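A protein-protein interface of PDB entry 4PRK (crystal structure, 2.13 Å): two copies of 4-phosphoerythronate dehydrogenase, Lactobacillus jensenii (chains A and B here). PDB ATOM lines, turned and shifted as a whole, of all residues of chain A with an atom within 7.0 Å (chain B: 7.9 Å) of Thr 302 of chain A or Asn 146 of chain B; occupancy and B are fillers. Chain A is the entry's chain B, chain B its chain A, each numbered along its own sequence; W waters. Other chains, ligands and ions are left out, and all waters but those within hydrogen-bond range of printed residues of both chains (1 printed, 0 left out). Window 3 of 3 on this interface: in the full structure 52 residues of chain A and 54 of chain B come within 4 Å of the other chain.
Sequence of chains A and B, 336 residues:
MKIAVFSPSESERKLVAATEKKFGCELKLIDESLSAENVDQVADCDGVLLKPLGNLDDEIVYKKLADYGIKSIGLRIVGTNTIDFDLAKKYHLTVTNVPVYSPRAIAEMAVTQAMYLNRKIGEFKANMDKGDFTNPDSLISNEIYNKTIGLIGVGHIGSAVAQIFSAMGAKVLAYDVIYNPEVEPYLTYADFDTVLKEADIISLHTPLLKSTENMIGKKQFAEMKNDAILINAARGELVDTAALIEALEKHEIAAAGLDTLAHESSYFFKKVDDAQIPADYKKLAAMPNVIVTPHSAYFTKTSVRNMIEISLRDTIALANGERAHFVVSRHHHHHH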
ATOM      1  N   TYR A 101     -19.280   8.908  28.578  1.00  0.00           N
ATOM      2  CA  TYR A 101     -18.059   9.670  28.487  1.00  0.00           C
ATOM      3  C   TYR A 101     -17.261   9.228  27.272  1.00  0.00           C
ATOM      4  O   TYR A 101     -17.066   9.982  26.338  1.00  0.00           O
ATOM      5  CB  TYR A 101     -17.200   9.375  29.708  1.00  0.00           C
ATOM      6  CG  TYR A 101     -17.805   9.641  31.067  1.00  0.00           C
ATOM      7  CD1 TYR A 101     -18.687  10.688  31.280  1.00  0.00           C
ATOM      8  CD2 TYR A 101     -17.452   8.864  32.152  1.00  0.00           C
ATOM      9  CE1 TYR A 101     -19.214  10.934  32.536  1.00  0.00           C
ATOM     10  CE2 TYR A 101     -17.967   9.107  33.409  1.00  0.00           C
ATOM     11  CZ  TYR A 101     -18.851  10.136  33.595  1.00  0.00           C
ATOM     12  OH  TYR A 101     -19.353  10.353  34.851  1.00  0.00           O
ATOM     13  N   SER A 102     -16.774   7.998  27.322  1.00  0.00           N
ATOM     14  CA  SER A 102     -16.201   7.300  26.188  1.00  0.00           C
ATOM     15  C   SER A 102     -16.273   5.829  26.512  1.00  0.00           C
ATOM     16  O   SER A 102     -15.503   5.377  27.343  1.00  0.00           O
ATOM     17  CB  SER A 102     -14.743   7.690  26.010  1.00  0.00           C
ATOM     18  OG  SER A 102     -14.122   6.930  25.013  1.00  0.00           O
ATOM     19  N   ALA A 105     -12.916   4.018  26.345  1.00  0.00           N
ATOM     20  CA  ALA A 105     -11.944   4.314  27.357  1.00  0.00           C
ATOM     21  C   ALA A 105     -11.976   3.235  28.397  1.00  0.00           C
ATOM     22  O   ALA A 105     -10.961   2.715  28.767  1.00  0.00           O
ATOM     23  CB  ALA A 105     -12.196   5.699  27.944  1.00  0.00           C
ATOM     24  N   GLU A 108     -11.215  -0.391  26.764  1.00  0.00           N
ATOM     25  CA  GLU A 108      -9.785  -0.534  26.561  1.00  0.00           C
ATOM     26  C   GLU A 108      -8.989  -0.785  27.846  1.00  0.00           C
ATOM     27  O   GLU A 108      -8.047  -1.582  27.873  1.00  0.00           O
ATOM     28  CB  GLU A 108      -9.278   0.671  25.761  1.00  0.00           C
ATOM     29  CG  GLU A 108      -9.694   0.565  24.299  1.00  0.00           C
ATOM     30  CD  GLU A 108      -9.075   1.607  23.429  1.00  0.00           C
ATOM     31  OE1 GLU A 108      -7.978   2.118  23.729  1.00  0.00           O
ATOM     32  OE2 GLU A 108      -9.652   1.917  22.404  1.00  0.00           O
ATOM     33  N   TYR A 298     -12.051   5.461  32.864  1.00  0.00           N
ATOM     34  CA  TYR A 298     -12.613   6.570  32.086  1.00  0.00           C
ATOM     35  C   TYR A 298     -11.550   7.527  31.604  1.00  0.00           C
ATOM     36  O   TYR A 298     -11.769   8.286  30.640  1.00  0.00           O
ATOM     37  CB  TYR A 298     -13.659   7.371  32.918  1.00  0.00           C
ATOM     38  CG  TYR A 298     -12.989   8.318  33.897  1.00  0.00           C
ATOM     39  CD1 TYR A 298     -12.495   7.866  35.098  1.00  0.00           C
ATOM     40  CD2 TYR A 298     -12.751   9.642  33.545  1.00  0.00           C
ATOM     41  CE1 TYR A 298     -11.834   8.724  35.955  1.00  0.00           C
ATOM     42  CE2 TYR A 298     -12.086  10.506  34.393  1.00  0.00           C
ATOM     43  CZ  TYR A 298     -11.621  10.046  35.588  1.00  0.00           C
ATOM     44  OH  TYR A 298     -10.935  10.938  36.416  1.00  0.00           O
ATOM     45  N   PHE A 299     -10.388   7.509  32.257  1.00  0.00           N
ATOM     46  CA  PHE A 299      -9.534   8.691  32.261  1.00  0.00           C
ATOM     47  C   PHE A 299      -8.695   8.878  30.964  1.00  0.00           C
ATOM     48  O   PHE A 299      -7.456   8.670  30.935  1.00  0.00           O
ATOM     49  CB  PHE A 299      -8.657   8.655  33.536  1.00  0.00           C
ATOM     50  CG  PHE A 299      -7.928   9.950  33.850  1.00  0.00           C
ATOM     51  CD1 PHE A 299      -8.492  11.193  33.593  1.00  0.00           C
ATOM     52  CD2 PHE A 299      -6.718   9.918  34.497  1.00  0.00           C
ATOM     53  CE1 PHE A 299      -7.815  12.367  33.888  1.00  0.00           C
ATOM     54  CE2 PHE A 299      -6.041  11.082  34.809  1.00  0.00           C
ATOM     55  CZ  PHE A 299      -6.596  12.306  34.503  1.00  0.00           C
ATOM     56  N   THR A 300      -9.366   9.302  29.890  1.00  0.00           N
ATOM     57  CA  THR A 300      -8.655   9.659  28.681  1.00  0.00           C
ATOM     58  C   THR A 300      -8.980  11.058  28.327  1.00  0.00           C
ATOM     59  O   THR A 300      -9.918  11.635  28.881  1.00  0.00           O
ATOM     60  CB  THR A 300      -9.076   8.780  27.526  1.00  0.00           C
ATOM     61  OG1 THR A 300     -10.480   8.970  27.277  1.00  0.00           O
ATOM     62  CG2 THR A 300      -8.819   7.393  27.885  1.00  0.00           C
ATOM     63  N   LYS A 301      -8.209  11.591  27.388  1.00  0.00           N
ATOM     64  CA  LYS A 301      -8.419  12.934  26.841  1.00  0.00           C
ATOM     65  C   LYS A 301      -9.837  13.088  26.276  1.00  0.00           C
ATOM     66  O   LYS A 301     -10.478  14.127  26.395  1.00  0.00           O
ATOM     67  CB  LYS A 301      -7.435  13.185  25.724  1.00  0.00           C
ATOM     68  CG  LYS A 301      -5.999  13.151  26.211  1.00  0.00           C
ATOM     69  CD  LYS A 301      -5.049  13.879  25.280  1.00  0.00           C
ATOM     70  CE  LYS A 301      -3.687  14.016  25.951  1.00  0.00           C
ATOM     71  NZ  LYS A 301      -3.451  15.399  26.426  1.00  0.00           N
ATOM     72  N   THR A 302     -10.296  12.043  25.614  1.00  0.00           N
ATOM     73  CA  THR A 302     -11.629  12.034  25.026  1.00  0.00           C
ATOM     74  C   THR A 302     -12.717  12.149  26.096  1.00  0.00           C
ATOM     75  O   THR A 302     -13.635  12.931  25.943  1.00  0.00           O
ATOM     76  CB  THR A 302     -11.849  10.733  24.245  1.00  0.00           C
ATOM     77  OG1 THR A 302     -10.798  10.577  23.256  1.00  0.00           O
ATOM     78  CG2 THR A 302     -13.237  10.740  23.600  1.00  0.00           C
ATOM     79  N   SER A 303     -12.590  11.386  27.178  1.00  0.00           N
ATOM     80  CA  SER A 303     -13.612  11.393  28.211  1.00  0.00           C
ATOM     81  C   SER A 303     -13.622  12.738  28.878  1.00  0.00           C
ATOM     82  O   SER A 303     -14.676  13.305  29.121  1.00  0.00           O
ATOM     83  CB  SER A 303     -13.350  10.344  29.281  1.00  0.00           C
ATOM     84  OG  SER A 303     -13.463   9.047  28.756  1.00  0.00           O
ATOM     85  N   VAL A 304     -12.436  13.252  29.177  1.00  0.00           N
ATOM     86  CA  VAL A 304     -12.331  14.550  29.825  1.00  0.00           C
ATOM     87  C   VAL A 304     -12.947  15.615  28.923  1.00  0.00           C
ATOM     88  O   VAL A 304     -13.760  16.396  29.372  1.00  0.00           O
ATOM     89  CB  VAL A 304     -10.864  14.858  30.235  1.00  0.00           C
ATOM     90  CG1 VAL A 304     -10.670  16.327  30.642  1.00  0.00           C
ATOM     91  CG2 VAL A 304     -10.452  13.939  31.362  1.00  0.00           C
ATOM     92  N   ARG A 305     -12.606  15.606  27.638  1.00  0.00           N
ATOM     93  CA  ARG A 305     -13.200  16.553  26.679  1.00  0.00           C
ATOM     94  C   ARG A 305     -14.732  16.458  26.593  1.00  0.00           C
ATOM     95  O   ARG A 305     -15.423  17.493  26.529  1.00  0.00           O
ATOM     96  CB  ARG A 305     -12.591  16.379  25.268  1.00  0.00           C
ATOM     97  CG  ARG A 305     -13.158  17.333  24.234  1.00  0.00           C
ATOM     98  CD  ARG A 305     -12.516  17.179  22.870  1.00  0.00           C
ATOM     99  NE  ARG A 305     -12.688  15.868  22.233  1.00  0.00           N
ATOM    100  CZ  ARG A 305     -13.851  15.348  21.827  1.00  0.00           C
ATOM    101  NH1 ARG A 305     -14.997  15.989  22.021  1.00  0.00           N
ATOM    102  NH2 ARG A 305     -13.873  14.163  21.237  1.00  0.00           N
ATOM    103  N   ASN A 306     -15.246  15.227  26.606  1.00  0.00           N
ATOM    104  CA  ASN A 306     -16.677  15.007  26.431  1.00  0.00           C
ATOM    105  C   ASN A 306     -17.450  15.414  27.634  1.00  0.00           C
ATOM    106  O   ASN A 306     -18.433  16.117  27.511  1.00  0.00           O
ATOM    107  CB  ASN A 306     -16.988  13.560  26.039  1.00  0.00           C
ATOM    108  CG  ASN A 306     -16.451  13.203  24.662  1.00  0.00           C
ATOM    109  OD1 ASN A 306     -16.105  14.077  23.867  1.00  0.00           O
ATOM    110  ND2 ASN A 306     -16.370  11.919  24.375  1.00  0.00           N
ATOM    111  N   MET A 307     -16.967  15.047  28.807  1.00  0.00           N
ATOM    112  CA  MET A 307     -17.571  15.522  30.050  1.00  0.00           C
ATOM    113  C   MET A 307     -17.746  17.021  30.074  1.00  0.00           C
ATOM    114  O   MET A 307     -18.774  17.542  30.519  1.00  0.00           O
ATOM    115  CB  MET A 307     -16.775  15.054  31.278  1.00  0.00           C
ATOM    116  CG  MET A 307     -16.913  13.547  31.570  1.00  0.00           C
ATOM    117  SD  MET A 307     -15.660  12.834  32.730  1.00  0.00           S
ATOM    118  CE  MET A 307     -16.217  13.615  34.233  1.00  0.00           C
ATOM    119  N   ILE A 308     -16.746  17.729  29.591  1.00  0.00           N
ATOM    120  CA  ILE A 308     -16.809  19.180  29.590  1.00  0.00           C
ATOM    121  C   ILE A 308     -17.743  19.665  28.499  1.00  0.00           C
ATOM    122  O   ILE A 308     -18.497  20.602  28.725  1.00  0.00           O
ATOM    123  CB  ILE A 308     -15.421  19.795  29.337  1.00  0.00           C
ATOM    124  CG1 ILE A 308     -14.615  19.822  30.614  1.00  0.00           C
ATOM    125  CG2 ILE A 308     -15.526  21.181  28.762  1.00  0.00           C
ATOM    126  CD1 ILE A 308     -14.900  21.023  31.489  1.00  0.00           C
ATOM    127  N   ILE B 140      -3.064  11.022  32.609  1.00  0.00           N
ATOM    128  CA  ILE B 140      -4.176  10.872  31.653  1.00  0.00           C
ATOM    129  C   ILE B 140      -3.740   9.974  30.507  1.00  0.00           C
ATOM    130  O   ILE B 140      -2.578   9.910  30.151  1.00  0.00           O
ATOM    131  CB  ILE B 140      -4.653  12.231  31.145  1.00  0.00           C
ATOM    132  CG1 ILE B 140      -6.062  12.121  30.559  1.00  0.00           C
ATOM    133  CG2 ILE B 140      -3.687  12.851  30.152  1.00  0.00           C
ATOM    134  CD1 ILE B 140      -6.660  13.484  30.278  1.00  0.00           C
ATOM    135  N   SER B 141      -4.678   9.235  29.952  1.00  0.00           N
ATOM    136  CA  SER B 141      -4.371   8.276  28.912  1.00  0.00           C
ATOM    137  C   SER B 141      -5.112   8.630  27.641  1.00  0.00           C
ATOM    138  O   SER B 141      -5.582   9.729  27.499  1.00  0.00           O
ATOM    139  CB  SER B 141      -4.681   6.856  29.366  1.00  0.00           C
ATOM    140  OG  SER B 141      -4.097   5.911  28.512  1.00  0.00           O
ATOM    141  N   ASN B 142      -5.160   7.706  26.700  1.00  0.00           N
ATOM    142  CA  ASN B 142      -5.853   7.952  25.444  1.00  0.00           C
ATOM    143  C   ASN B 142      -6.316   6.637  24.762  1.00  0.00           C
ATOM    144  O   ASN B 142      -5.792   5.557  25.062  1.00  0.00           O
ATOM    145  CB  ASN B 142      -5.022   8.800  24.496  1.00  0.00           C
ATOM    146  CG  ASN B 142      -5.895   9.569  23.471  1.00  0.00           C
ATOM    147  OD1 ASN B 142      -7.137   9.544  23.532  1.00  0.00           O
ATOM    148  ND2 ASN B 142      -5.249  10.246  22.541  1.00  0.00           N
ATOM    149  N   GLU B 143      -7.333   6.741  23.903  1.00  0.00           N
ATOM    150  CA  GLU B 143      -7.888   5.559  23.296  1.00  0.00           C
ATOM    151  C   GLU B 143      -6.930   5.191  22.204  1.00  0.00           C
ATOM    152  O   GLU B 143      -6.303   6.044  21.581  1.00  0.00           O
ATOM    153  CB  GLU B 143      -9.310   5.744  22.754  1.00  0.00           C
ATOM    154  CG  GLU B 143     -10.390   5.833  23.816  1.00  0.00           C
ATOM    155  CD  GLU B 143     -10.569   7.248  24.381  1.00  0.00           C
ATOM    156  OE1 GLU B 143      -9.906   8.176  23.863  1.00  0.00           O
ATOM    157  OE2 GLU B 143     -11.416   7.439  25.289  1.00  0.00           O
ATOM    158  N   ILE B 144      -6.846   3.904  21.946  1.00  0.00           N
ATOM    159  CA  ILE B 144      -5.875   3.401  21.037  1.00  0.00           C
ATOM    160  C   ILE B 144      -6.196   3.838  19.610  1.00  0.00           C
ATOM    161  O   ILE B 144      -5.261   4.095  18.831  1.00  0.00           O
ATOM    162  CB  ILE B 144      -5.728   1.867  21.222  1.00  0.00           C
ATOM    163  CG1 ILE B 144      -4.443   1.381  20.624  1.00  0.00           C
ATOM    164  CG2 ILE B 144      -6.903   1.127  20.625  1.00  0.00           C
ATOM    165  CD1 ILE B 144      -3.274   1.648  21.547  1.00  0.00           C
ATOM    166  N   TYR B 145      -7.482   4.018  19.264  1.00  0.00           N
ATOM    167  CA  TYR B 145      -7.826   4.576  17.937  1.00  0.00           C
ATOM    168  C   TYR B 145      -7.416   6.044  17.800  1.00  0.00           C
ATOM    169  O   TYR B 145      -7.627   6.646  16.748  1.00  0.00           O
ATOM    170  CB  TYR B 145      -9.360   4.430  17.570  1.00  0.00           C
ATOM    171  CG  TYR B 145     -10.310   5.075  18.541  1.00  0.00           C
ATOM    172  CD1 TYR B 145     -10.628   6.419  18.478  1.00  0.00           C
ATOM    173  CD2 TYR B 145     -10.865   4.335  19.536  1.00  0.00           C
ATOM    174  CE1 TYR B 145     -11.506   6.971  19.399  1.00  0.00           C
ATOM    175  CE2 TYR B 145     -11.693   4.866  20.443  1.00  0.00           C
ATOM    176  CZ  TYR B 145     -12.006   6.182  20.389  1.00  0.00           C
ATOM    177  OH  TYR B 145     -12.869   6.622  21.344  1.00  0.00           O
ATOM    178  N   ASN B 146      -6.831   6.667  18.809  1.00  0.00           N
ATOM    179  CA  ASN B 146      -6.288   8.021  18.548  1.00  0.00           C
ATOM    180  C   ASN B 146      -4.783   8.029  18.353  1.00  0.00           C
ATOM    181  O   ASN B 146      -4.209   9.069  18.151  1.00  0.00           O
ATOM    182  CB  ASN B 146      -6.674   8.976  19.654  1.00  0.00           C
ATOM    183  CG  ASN B 146      -8.155   9.224  19.687  1.00  0.00           C
ATOM    184  OD1 ASN B 146      -8.808   9.150  20.723  1.00  0.00           O
ATOM    185  ND2 ASN B 146      -8.687   9.517  18.543  1.00  0.00           N
ATOM    186  N   LYS B 147      -4.159   6.870  18.386  1.00  0.00           N
ATOM    187  CA  LYS B 147      -2.709   6.777  18.384  1.00  0.00           C
ATOM    188  C   LYS B 147      -2.228   6.344  17.032  1.00  0.00           C
ATOM    189  O   LYS B 147      -2.971   5.672  16.278  1.00  0.00           O
ATOM    190  CB  LYS B 147      -2.305   5.749  19.443  1.00  0.00           C
ATOM    191  CG  LYS B 147      -2.572   6.203  20.868  1.00  0.00           C
ATOM    192  CD  LYS B 147      -1.270   6.359  21.615  1.00  0.00           C
ATOM    193  CE  LYS B 147      -1.396   6.900  23.026  1.00  0.00           C
ATOM    194  NZ  LYS B 147      -1.070   8.341  22.995  1.00  0.00           N
ATOM    195  N   THR B 148      -0.964   6.647  16.750  1.00  0.00           N
ATOM    196  CA  THR B 148      -0.246   6.160  15.602  1.00  0.00           C
ATOM    197  C   THR B 148       0.788   5.155  16.085  1.00  0.00           C
ATOM    198  O   THR B 148       1.552   5.405  17.029  1.00  0.00           O
ATOM    199  CB  THR B 148       0.502   7.304  14.881  1.00  0.00           C
ATOM    200  OG1 THR B 148      -0.438   8.183  14.268  1.00  0.00           O
ATOM    201  CG2 THR B 148       1.376   6.769  13.788  1.00  0.00           C
ATOM    202  N   ILE B 149       0.843   4.023  15.391  1.00  0.00           N
ATOM    203  CA  ILE B 149       1.745   2.964  15.719  1.00  0.00           C
ATOM    204  C   ILE B 149       2.792   3.033  14.658  1.00  0.00           C
ATOM    205  O   ILE B 149       2.481   3.257  13.471  1.00  0.00           O
ATOM    206  CB  ILE B 149       1.079   1.584  15.568  1.00  0.00           C
ATOM    207  CG1 ILE B 149      -0.312   1.554  16.223  1.00  0.00           C
ATOM    208  CG2 ILE B 149       2.014   0.521  16.041  1.00  0.00           C
ATOM    209  CD1 ILE B 149      -0.345   1.671  17.757  1.00  0.00           C
ATOM    210  N   MET B 168      -8.167  -2.354  16.203  1.00  0.00           N
ATOM    211  CA  MET B 168      -8.670  -1.480  17.275  1.00  0.00           C
ATOM    212  C   MET B 168      -8.898  -0.020  16.802  1.00  0.00           C
ATOM    213  O   MET B 168      -9.386   0.850  17.568  1.00  0.00           O
ATOM    214  CB  MET B 168      -7.705  -1.477  18.458  1.00  0.00           C
ATOM    215  CG  MET B 168      -7.411  -2.848  19.019  1.00  0.00           C
ATOM    216  SD  MET B 168      -6.542  -2.825  20.589  1.00  0.00           S
ATOM    217  CE  MET B 168      -4.877  -3.026  20.102  1.00  0.00           C
ATOM    218  N   GLY B 169      -8.564   0.254  15.551  1.00  0.00           N
ATOM    219  CA  GLY B 169      -8.774   1.567  14.972  1.00  0.00           C
ATOM    220  C   GLY B 169      -7.540   2.472  14.932  1.00  0.00           C
ATOM    221  O   GLY B 169      -7.619   3.595  14.424  1.00  0.00           O
ATOM    222  N   ALA B 170      -6.388   2.005  15.422  1.00  0.00           N
ATOM    223  CA  ALA B 170      -5.172   2.806  15.340  1.00  0.00           C
ATOM    224  C   ALA B 170      -4.698   3.013  13.914  1.00  0.00           C
ATOM    225  O   ALA B 170      -4.927   2.177  13.055  1.00  0.00           O
ATOM    226  CB  ALA B 170      -4.051   2.172  16.138  1.00  0.00           C
ATOM    227  N   LYS B 171      -3.969   4.099  13.676  1.00  0.00           N
ATOM    228  CA  LYS B 171      -3.262   4.249  12.420  1.00  0.00           C
ATOM    229  C   LYS B 171      -1.886   3.609  12.550  1.00  0.00           C
ATOM    230  O   LYS B 171      -1.152   3.919  13.485  1.00  0.00           O
ATOM    231  CB  LYS B 171      -3.126   5.736  12.046  1.00  0.00           C
ATOM    232  CG  LYS B 171      -2.370   5.943  10.743  1.00  0.00           C
ATOM    233  CD  LYS B 171      -1.715   7.294  10.693  1.00  0.00           C
ATOM    234  CE  LYS B 171      -2.383   8.271   9.755  1.00  0.00           C
ATOM    235  NZ  LYS B 171      -1.313   9.170   9.208  1.00  0.00           N
ATOM    236  N   ASP B 200       3.196   7.358  18.032  1.00  0.00           N
ATOM    237  CA  ASP B 200       3.067   7.426  19.504  1.00  0.00           C
ATOM    238  C   ASP B 200       3.503   6.136  20.185  1.00  0.00           C
ATOM    239  O   ASP B 200       3.818   6.144  21.384  1.00  0.00           O
ATOM    240  CB  ASP B 200       1.645   7.718  19.924  1.00  0.00           C
ATOM    241  CG  ASP B 200       1.076   8.907  19.216  1.00  0.00           C
ATOM    242  OD1 ASP B 200       1.657   9.993  19.322  1.00  0.00           O
ATOM    243  OD2 ASP B 200       0.044   8.741  18.562  1.00  0.00           O
ATOM    244  N   LYS B 225       8.600  11.270  19.687  1.00  0.00           N
ATOM    245  CA  LYS B 225       7.771  12.187  20.470  1.00  0.00           C
ATOM    246  C   LYS B 225       8.078  11.964  21.965  1.00  0.00           C
ATOM    247  O   LYS B 225       8.456  10.844  22.384  1.00  0.00           O
ATOM    248  CB  LYS B 225       6.299  11.957  20.120  1.00  0.00           C
ATOM    249  CG  LYS B 225       6.079  12.206  18.654  1.00  0.00           C
ATOM    250  CD  LYS B 225       4.818  11.604  18.108  1.00  0.00           C
ATOM    251  CE  LYS B 225       3.611  12.253  18.676  1.00  0.00           C
ATOM    252  NZ  LYS B 225       2.505  11.856  17.750  1.00  0.00           N
HETATM  253  O   HOH W   1      -6.804   3.015  25.920  1.00  0.00           O
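Of chain B, only Asn 142, Glu 143 and Asn 146 come within 4 Å of Thr 302 of chain A. Of the printed residues of chain A, Ile 140 of chain B touches Phe 299, Thr 300, Lys 301 and Val 304. Of the printed residues of chain B, Glu 108 of chain A touches Glu 143, Ile 144 and Tyr 145. Of the printed residues of chain A, Glu 143 of chain B touches Ser 102, Ala 105, Glu 108, Thr 300 and Thr 302. Gly 169 of chain B touches none of the printed residues of chain A. Ile 308 of chain A touches none of the printed residues of chain B.
Printed residues of chain A that touch a printed residue of chain B: Ser 102, Ala 105, Glu 108, Phe 299, Thr 300, Lys 301, Thr 302 and Val 304. Hydrophobic or aromatic side chains of chain A within 4 Å of the printed part of chain B: Ala 105, Phe 299 and Val 304. Hydrophobic or aromatic side chains of chain B that line the printed part of chain A: Ile 140, Ile 144 and Tyr 145. Among the printed residues, 18 pairs touch across the chains. Among the printed residues, no Asp or Glu carboxylate lies within 4 Å of a Lys or Arg side-chain nitrogen of the other chain.
No position is printed for both chains. Of the 18 pairs that touch across the chains among the printed residues, none has its exchanged pair printed and touching as well.
Water W1 lies within hydrogen-bond range of the side-chain carboxylate of Glu 108 of chain A (2.6 Å) and the backbone carbonyl oxygen of Asn 142 of chain B (2.9 Å).
Among the printed residues, merely in contact across the chains: Ala 105 of chain A with Glu 143 of chain B, Thr 300 of chain A with Ser 141 of chain B, Glu 108 of chain A with Glu 143 of chain B, Thr 302 of chain A with Asn 146 of chain B, Phe 299 of chain A with Ile 140 of chain B, Lys 301 of chain A with Ile 140 of chain B, Thr 302 of chain A with Asn 142 of chain B, Thr 300 of chain A with Ile 140 of chain B, Thr 300 of chain A with Asn 142 of chain B, Ser 102 of chain A with Tyr 145 of chain B, Glu 108 of chain A with Tyr 145 of chain B and Val 304 of chain A with Ile 140 of chain B.
OG1 of Thr 300 of chain A sits at hydrogen-bond distance from OE2 of Glu 143 of chain B (2.7 Å). N of Ser 141 of chain B sits at hydrogen-bond distance from O of Phe 299 of chain A, 3.0 Å away. O of Ser 141 of chain B sits at hydrogen-bond distance from N of Lys 301 of chain A (3.2 Å). The side-chain hydroxyl (OG1) of Thr 302 of chain A is in hydrogen-bond range of the side-chain carboxylate (OE1) of Glu 143 of chain B (2.6 Å). N of Ile 144 of chain B is in hydrogen-bond range of OE1 of Glu 108 of chain A, at 2.8 Å. OE2 of Glu 143 of chain B lies within hydrogen-bond range of OG of Ser 102 of chain A.
The side-chain hydroxyl (OG1) of Thr 300 of chain A sits close to the backbone NH (N) of Thr 302 of chain A (3.5 Å). OD1 of Asn 142 of chain B sits close to OE1 of Glu 143 of chain B. The side-chain amide oxygen (OD1) of Asn 146 of chain B sits close to the side-chain amide oxygen (OD1) of Asn 142 of chain B, 3.3 Å away. O of Thr 302 of chain A sits close to ND2 of Asn 306 of chain A, 3.3 Å away. The side-chain hydroxyl (OG1) of Thr 300 of chain A sits at hydrogen-bond distance from the backbone NH (N) of Ser 303 of chain A (3.2 Å). N of Ala 105 of chain A sits at hydrogen-bond distance from OG of Ser 102 of chain A, 3.4 Å away.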
